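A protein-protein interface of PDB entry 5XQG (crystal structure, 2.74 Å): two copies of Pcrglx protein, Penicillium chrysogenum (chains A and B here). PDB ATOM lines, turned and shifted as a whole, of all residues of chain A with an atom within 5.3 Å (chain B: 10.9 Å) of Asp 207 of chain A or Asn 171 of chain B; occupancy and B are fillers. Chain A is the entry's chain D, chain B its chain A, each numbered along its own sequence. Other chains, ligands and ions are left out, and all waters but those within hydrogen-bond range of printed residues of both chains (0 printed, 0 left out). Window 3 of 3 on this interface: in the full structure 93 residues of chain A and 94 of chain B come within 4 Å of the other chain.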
ATOM      1  N   TYR A 176      17.943  29.500   3.019  1.00  0.00           N
ATOM      2  CA  TYR A 176      18.190  28.619   1.885  1.00  0.00           C
ATOM      3  C   TYR A 176      17.016  28.550   0.939  1.00  0.00           C
ATOM      4  O   TYR A 176      15.868  28.595   1.360  1.00  0.00           O
ATOM      5  CB  TYR A 176      18.511  27.203   2.355  1.00  0.00           C
ATOM      6  CG  TYR A 176      19.841  27.111   3.018  1.00  0.00           C
ATOM      7  CD1 TYR A 176      21.006  27.028   2.254  1.00  0.00           C
ATOM      8  CD2 TYR A 176      19.952  27.152   4.404  1.00  0.00           C
ATOM      9  CE1 TYR A 176      22.256  26.963   2.858  1.00  0.00           C
ATOM     10  CE2 TYR A 176      21.191  27.073   5.021  1.00  0.00           C
ATOM     11  CZ  TYR A 176      22.341  26.972   4.242  1.00  0.00           C
ATOM     12  OH  TYR A 176      23.573  26.924   4.844  1.00  0.00           O
ATOM     13  N   SER A 177      17.329  28.400  -0.341  1.00  0.00           N
ATOM     14  CA  SER A 177      16.340  28.300  -1.368  1.00  0.00           C
ATOM     15  C   SER A 177      16.774  27.213  -2.349  1.00  0.00           C
ATOM     16  O   SER A 177      17.878  27.281  -2.862  1.00  0.00           O
ATOM     17  CB  SER A 177      16.260  29.651  -2.072  1.00  0.00           C
ATOM     18  OG  SER A 177      16.276  30.733  -1.156  1.00  0.00           O
ATOM     19  N   ASN A 178      15.939  26.198  -2.573  1.00  0.00           N
ATOM     20  CA  ASN A 178      16.156  25.224  -3.676  1.00  0.00           C
ATOM     21  C   ASN A 178      15.353  25.594  -4.908  1.00  0.00           C
ATOM     22  O   ASN A 178      14.291  26.247  -4.849  1.00  0.00           O
ATOM     23  CB  ASN A 178      15.756  23.775  -3.338  1.00  0.00           C
ATOM     24  CG  ASN A 178      16.278  23.309  -2.013  1.00  0.00           C
ATOM     25  OD1 ASN A 178      17.285  23.797  -1.497  1.00  0.00           O
ATOM     26  ND2 ASN A 178      15.582  22.346  -1.439  1.00  0.00           N
ATOM     27  N   VAL A 205      12.191  28.439  -8.171  1.00  0.00           N
ATOM     28  CA  VAL A 205      11.992  27.895  -6.799  1.00  0.00           C
ATOM     29  C   VAL A 205      11.181  26.636  -6.712  1.00  0.00           C
ATOM     30  O   VAL A 205      10.271  26.416  -7.492  1.00  0.00           O
ATOM     31  CB  VAL A 205      11.255  28.809  -5.775  1.00  0.00           C
ATOM     32  CG1 VAL A 205      12.259  29.387  -4.778  1.00  0.00           C
ATOM     33  CG2 VAL A 205      10.367  29.864  -6.429  1.00  0.00           C
ATOM     34  N   THR A 206      11.538  25.840  -5.717  1.00  0.00           N
ATOM     35  CA  THR A 206      10.749  24.702  -5.230  1.00  0.00           C
ATOM     36  C   THR A 206      10.598  24.930  -3.719  1.00  0.00           C
ATOM     37  O   THR A 206       9.776  25.702  -3.306  1.00  0.00           O
ATOM     38  CB  THR A 206      11.437  23.354  -5.575  1.00  0.00           C
ATOM     39  OG1 THR A 206      12.810  23.387  -5.155  1.00  0.00           O
ATOM     40  CG2 THR A 206      11.400  23.120  -7.067  1.00  0.00           C
ATOM     41  N   ASP A 207      11.446  24.347  -2.895  1.00  0.00           N
ATOM     42  CA  ASP A 207      11.362  24.560  -1.444  1.00  0.00           C
ATOM     43  C   ASP A 207      12.072  25.854  -1.026  1.00  0.00           C
ATOM     44  O   ASP A 207      12.792  26.484  -1.800  1.00  0.00           O
ATOM     45  CB  ASP A 207      11.977  23.358  -0.691  1.00  0.00           C
ATOM     46  CG  ASP A 207      11.199  22.047  -0.904  1.00  0.00           C
ATOM     47  OD1 ASP A 207      11.041  21.563  -2.055  1.00  0.00           O
ATOM     48  OD2 ASP A 207      10.759  21.476   0.110  1.00  0.00           O
ATOM     49  N   GLY A 208      11.873  26.226   0.229  1.00  0.00           N
ATOM     50  CA  GLY A 208      12.629  27.305   0.836  1.00  0.00           C
ATOM     51  C   GLY A 208      12.118  28.691   0.508  1.00  0.00           C
ATOM     52  O   GLY A 208      10.994  28.869   0.054  1.00  0.00           O
ATOM     53  N   THR A 209      12.977  29.673   0.744  1.00  0.00           N
ATOM     54  CA  THR A 209      12.599  31.077   0.755  1.00  0.00           C
ATOM     55  C   THR A 209      12.408  31.569  -0.696  1.00  0.00           C
ATOM     56  O   THR A 209      13.131  31.132  -1.612  1.00  0.00           O
ATOM     57  CB  THR A 209      13.617  31.891   1.591  1.00  0.00           C
ATOM     58  OG1 THR A 209      13.068  33.140   1.947  1.00  0.00           O
ATOM     59  CG2 THR A 209      14.875  32.163   0.853  1.00  0.00           C
ATOM     60  N   SER B 161      20.602  21.051  15.665  1.00  0.00           N
ATOM     61  CA  SER B 161      20.138  19.946  14.847  1.00  0.00           C
ATOM     62  C   SER B 161      20.841  19.937  13.514  1.00  0.00           C
ATOM     63  O   SER B 161      21.596  20.836  13.198  1.00  0.00           O
ATOM     64  CB  SER B 161      18.635  20.052  14.607  1.00  0.00           C
ATOM     65  OG  SER B 161      18.370  20.808  13.433  1.00  0.00           O
ATOM     66  N   VAL B 162      20.536  18.921  12.714  1.00  0.00           N
ATOM     67  CA  VAL B 162      21.178  18.695  11.441  1.00  0.00           C
ATOM     68  C   VAL B 162      20.130  18.347  10.375  1.00  0.00           C
ATOM     69  O   VAL B 162      19.217  17.569  10.624  1.00  0.00           O
ATOM     70  CB  VAL B 162      22.287  17.617  11.626  1.00  0.00           C
ATOM     71  CG1 VAL B 162      22.206  16.466  10.620  1.00  0.00           C
ATOM     72  CG2 VAL B 162      23.665  18.291  11.596  1.00  0.00           C
ATOM     73  N   PRO B 163      20.265  18.916   9.167  1.00  0.00           N
ATOM     74  CA  PRO B 163      19.332  18.496   8.106  1.00  0.00           C
ATOM     75  C   PRO B 163      19.601  17.075   7.621  1.00  0.00           C
ATOM     76  O   PRO B 163      20.723  16.629   7.666  1.00  0.00           O
ATOM     77  CB  PRO B 163      19.572  19.523   7.015  1.00  0.00           C
ATOM     78  CG  PRO B 163      20.158  20.709   7.743  1.00  0.00           C
ATOM     79  CD  PRO B 163      21.046  20.097   8.769  1.00  0.00           C
ATOM     80  N   ASP B 164      18.567  16.363   7.198  1.00  0.00           N
ATOM     81  CA  ASP B 164      18.703  15.002   6.666  1.00  0.00           C
ATOM     82  C   ASP B 164      19.700  14.931   5.488  1.00  0.00           C
ATOM     83  O   ASP B 164      20.370  13.908   5.274  1.00  0.00           O
ATOM     84  CB  ASP B 164      17.346  14.495   6.133  1.00  0.00           C
ATOM     85  CG  ASP B 164      16.324  14.214   7.225  1.00  0.00           C
ATOM     86  OD1 ASP B 164      16.574  14.548   8.396  1.00  0.00           O
ATOM     87  OD2 ASP B 164      15.261  13.651   6.884  1.00  0.00           O
ATOM     88  N   ASN B 165      19.740  16.002   4.697  1.00  0.00           N
ATOM     89  CA  ASN B 165      20.598  16.078   3.519  1.00  0.00           C
ATOM     90  C   ASN B 165      20.674  17.543   3.077  1.00  0.00           C
ATOM     91  O   ASN B 165      20.129  18.404   3.748  1.00  0.00           O
ATOM     92  CB  ASN B 165      20.072  15.151   2.426  1.00  0.00           C
ATOM     93  CG  ASN B 165      18.594  15.317   2.194  1.00  0.00           C
ATOM     94  OD1 ASN B 165      17.801  14.431   2.459  1.00  0.00           O
ATOM     95  ND2 ASN B 165      18.218  16.446   1.705  1.00  0.00           N
ATOM     96  N   PHE B 166      21.342  17.837   1.967  1.00  0.00           N
ATOM     97  CA  PHE B 166      21.603  19.227   1.554  1.00  0.00           C
ATOM     98  C   PHE B 166      20.305  19.931   1.138  1.00  0.00           C
ATOM     99  O   PHE B 166      20.080  21.092   1.482  1.00  0.00           O
ATOM    100  CB  PHE B 166      22.617  19.255   0.398  1.00  0.00           C
ATOM    101  CG  PHE B 166      23.976  18.635   0.717  1.00  0.00           C
ATOM    102  CD1 PHE B 166      24.664  18.944   1.906  1.00  0.00           C
ATOM    103  CD2 PHE B 166      24.591  17.763  -0.203  1.00  0.00           C
ATOM    104  CE1 PHE B 166      25.905  18.406   2.171  1.00  0.00           C
ATOM    105  CE2 PHE B 166      25.840  17.228   0.051  1.00  0.00           C
ATOM    106  CZ  PHE B 166      26.494  17.560   1.234  1.00  0.00           C
ATOM    107  N   ASP B 167      19.476  19.217   0.384  1.00  0.00           N
ATOM    108  CA  ASP B 167      18.108  19.642   0.048  1.00  0.00           C
ATOM    109  C   ASP B 167      17.236  20.034   1.258  1.00  0.00           C
ATOM    110  O   ASP B 167      16.461  20.986   1.166  1.00  0.00           O
ATOM    111  CB  ASP B 167      17.373  18.554  -0.779  1.00  0.00           C
ATOM    112  CG  ASP B 167      17.877  18.452  -2.222  1.00  0.00           C
ATOM    113  OD1 ASP B 167      19.097  18.648  -2.472  1.00  0.00           O
ATOM    114  OD2 ASP B 167      17.020  18.143  -3.091  1.00  0.00           O
ATOM    115  N   ASN B 168      17.394  19.344   2.386  1.00  0.00           N
ATOM    116  CA  ASN B 168      16.583  19.581   3.575  1.00  0.00           C
ATOM    117  C   ASN B 168      16.934  20.918   4.286  1.00  0.00           C
ATOM    118  O   ASN B 168      16.230  21.338   5.199  1.00  0.00           O
ATOM    119  CB  ASN B 168      16.733  18.388   4.566  1.00  0.00           C
ATOM    120  CG  ASN B 168      15.582  18.281   5.597  1.00  0.00           C
ATOM    121  OD1 ASN B 168      15.815  17.911   6.753  1.00  0.00           O
ATOM    122  ND2 ASN B 168      14.338  18.555   5.172  1.00  0.00           N
ATOM    123  N   ARG B 169      18.021  21.583   3.904  1.00  0.00           N
ATOM    124  CA  ARG B 169      18.373  22.862   4.530  1.00  0.00           C
ATOM    125  C   ARG B 169      17.237  23.880   4.451  1.00  0.00           C
ATOM    126  O   ARG B 169      16.972  24.598   5.404  1.00  0.00           O
ATOM    127  CB  ARG B 169      19.610  23.453   3.862  1.00  0.00           C
ATOM    128  CG  ARG B 169      20.883  22.754   4.238  1.00  0.00           C
ATOM    129  CD  ARG B 169      21.975  23.168   3.299  1.00  0.00           C
ATOM    130  NE  ARG B 169      23.231  22.515   3.596  1.00  0.00           N
ATOM    131  CZ  ARG B 169      24.392  22.827   3.028  1.00  0.00           C
ATOM    132  NH1 ARG B 169      24.466  23.796   2.103  1.00  0.00           N
ATOM    133  NH2 ARG B 169      25.492  22.168   3.382  1.00  0.00           N
ATOM    134  N   ALA B 170      16.605  23.926   3.283  1.00  0.00           N
ATOM    135  CA  ALA B 170      15.464  24.796   2.998  1.00  0.00           C
ATOM    136  C   ALA B 170      14.264  24.612   3.932  1.00  0.00           C
ATOM    137  O   ALA B 170      13.516  25.533   4.139  1.00  0.00           O
ATOM    138  CB  ALA B 170      15.036  24.577   1.562  1.00  0.00           C
ATOM    139  N   ASN B 171      14.100  23.415   4.478  1.00  0.00           N
ATOM    140  CA  ASN B 171      12.953  23.037   5.297  1.00  0.00           C
ATOM    141  C   ASN B 171      13.345  22.596   6.686  1.00  0.00           C
ATOM    142  O   ASN B 171      12.542  21.990   7.373  1.00  0.00           O
ATOM    143  CB  ASN B 171      12.183  21.889   4.600  1.00  0.00           C
ATOM    144  CG  ASN B 171      11.277  22.391   3.473  1.00  0.00           C
ATOM    145  OD1 ASN B 171      10.633  23.454   3.589  1.00  0.00           O
ATOM    146  ND2 ASN B 171      11.208  21.624   2.381  1.00  0.00           N
ATOM    147  N   SER B 172      14.567  22.901   7.117  1.00  0.00           N
ATOM    148  CA  SER B 172      15.114  22.331   8.374  1.00  0.00           C
ATOM    149  C   SER B 172      16.058  23.343   9.000  1.00  0.00           C
ATOM    150  O   SER B 172      17.256  23.266   8.845  1.00  0.00           O
ATOM    151  CB  SER B 172      15.813  21.008   8.099  1.00  0.00           C
ATOM    152  OG  SER B 172      16.202  20.411   9.284  1.00  0.00           O
ATOM    153  N   PRO B 173      15.488  24.319   9.702  1.00  0.00           N
ATOM    154  CA  PRO B 173      16.327  25.438  10.080  1.00  0.00           C
ATOM    155  C   PRO B 173      17.314  24.967  11.136  1.00  0.00           C
ATOM    156  O   PRO B 173      17.012  23.990  11.841  1.00  0.00           O
ATOM    157  CB  PRO B 173      15.318  26.474  10.627  1.00  0.00           C
ATOM    158  CG  PRO B 173      14.119  25.679  11.043  1.00  0.00           C
ATOM    159  CD  PRO B 173      14.204  24.299  10.441  1.00  0.00           C
ATOM    160  N   ILE B 174      18.470  25.646  11.190  1.00  0.00           N
ATOM    161  CA  ILE B 174      19.591  25.341  12.091  1.00  0.00           C
ATOM    162  C   ILE B 174      19.807  26.537  13.059  1.00  0.00           C
ATOM    163  O   ILE B 174      20.001  27.648  12.581  1.00  0.00           O
ATOM    164  CB  ILE B 174      20.914  25.178  11.289  1.00  0.00           C
ATOM    165  CG1 ILE B 174      20.863  24.045  10.228  1.00  0.00           C
ATOM    166  CG2 ILE B 174      22.083  24.941  12.244  1.00  0.00           C
ATOM    167  CD1 ILE B 174      22.023  24.060   9.204  1.00  0.00           C
ATOM    168  N   GLN B 175      19.817  26.326  14.384  1.00  0.00           N
ATOM    169  CA  GLN B 175      20.131  27.400  15.387  1.00  0.00           C
ATOM    170  C   GLN B 175      21.627  27.315  15.874  1.00  0.00           C
ATOM    171  O   GLN B 175      22.002  26.440  16.661  1.00  0.00           O
ATOM    172  CB  GLN B 175      19.093  27.447  16.566  1.00  0.00           C
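Among the printed residues, merely in contact across the chains: Gly 208 of chain A with Ala 170 of chain B (3.7 Å), Tyr 176 of chain A with Arg 169 of chain B (3.8 Å), Asn 178 of chain A with Ala 170 of chain B (3.8 Å), Tyr 176 of chain A with Ala 170 of chain B (3.9 Å) and Asp 207 of chain A with Ala 170 of chain B (3.99 Å).
Of the printed residues of chain B, Tyr 176 of chain A touches Arg 169 (3.8 Å) and Ala 170 (3.9 Å).
Of chain B, only Asp 167 and Ala 170 come within 4 Å of Asn 178 of chain A.
No residue of chain B comes within 4 Å of Val 205 of chain A.
No residue of chain B comes within 4 Å of Thr 206 of chain A.
Phe 166 of chain B touches none of the printed residues of chain A.
Printed residues of chain A within 4 Å of Asp 167 of chain B: Asn 178 (3.1 Å).
Of the printed residues of chain A, Arg 169 of chain B touches Tyr 176 (3.8 Å).
Printed residues of chain A within 4 Å of Ala 170 of chain B: Tyr 176 (3.9 Å), Asn 178 (3.8 Å), Asp 207 (3.99 Å) and Gly 208 (3.7 Å).
Asn 171 of chain B touches one residue of chain A.
The nearest printed residue of chain B that does not touch Asp 207 of chain A is Asp 167 of chain B (5.4 Å).
The nearest residue of chain A that does not touch Asn 171 of chain B is Gly 208 of chain A (4.5 Å).
The backbone NH of Asp 167 of chain B lies close to the side-chain amide nitrogen of Asn 165 of chain B, at 3.3 Å.
The backbone carbonyl oxygen of Asn 178 of chain A is in hydrogen-bond range of the backbone NH of Thr 206 of chain A (2.9 Å).
The backbone carbonyl oxygen of Tyr 176 of chain A sits at hydrogen-bond distance from the backbone NH of Thr 209 of chain A, 3.1 Å away.
The backbone NH (N) of Asn 178 of chain A is in hydrogen-bond range of the backbone carbonyl oxygen (O) of Asp 207 of chain A (3.3 Å).
No position is printed for both chains.
Of the 7 pairs that touch across the chains among the printed residues, none has its exchanged pair printed and touching as well.
OD2 of Asp 207 of chain A lies close to ND2 of Asn 171 of chain B.
O of Asp 167 of chain B lies within hydrogen-bond range of ND2 of Asn 178 of chain A, 3.1 Å away.
Printed residues of chain B that touch a printed residue of chain A: Asp 167, Arg 169, Ala 170 and Asn 171.
Hydrophobic or aromatic side chains of chain B within 4 Å of the printed part of chain A: Ala 170.
Printed residues of chain A that touch a printed residue of chain B: Tyr 176, Asn 178, Asp 207 and Gly 208.
Hydrophobic or aromatic side chains of chain A within 4 Å of the printed part of chain B: Tyr 176.
Among the printed residues, 7 pairs touch across the chains.
Among the printed residues, no Asp or Glu carboxylate lies within 4 Å of a Lys or Arg side-chain nitrogen of the other chain.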
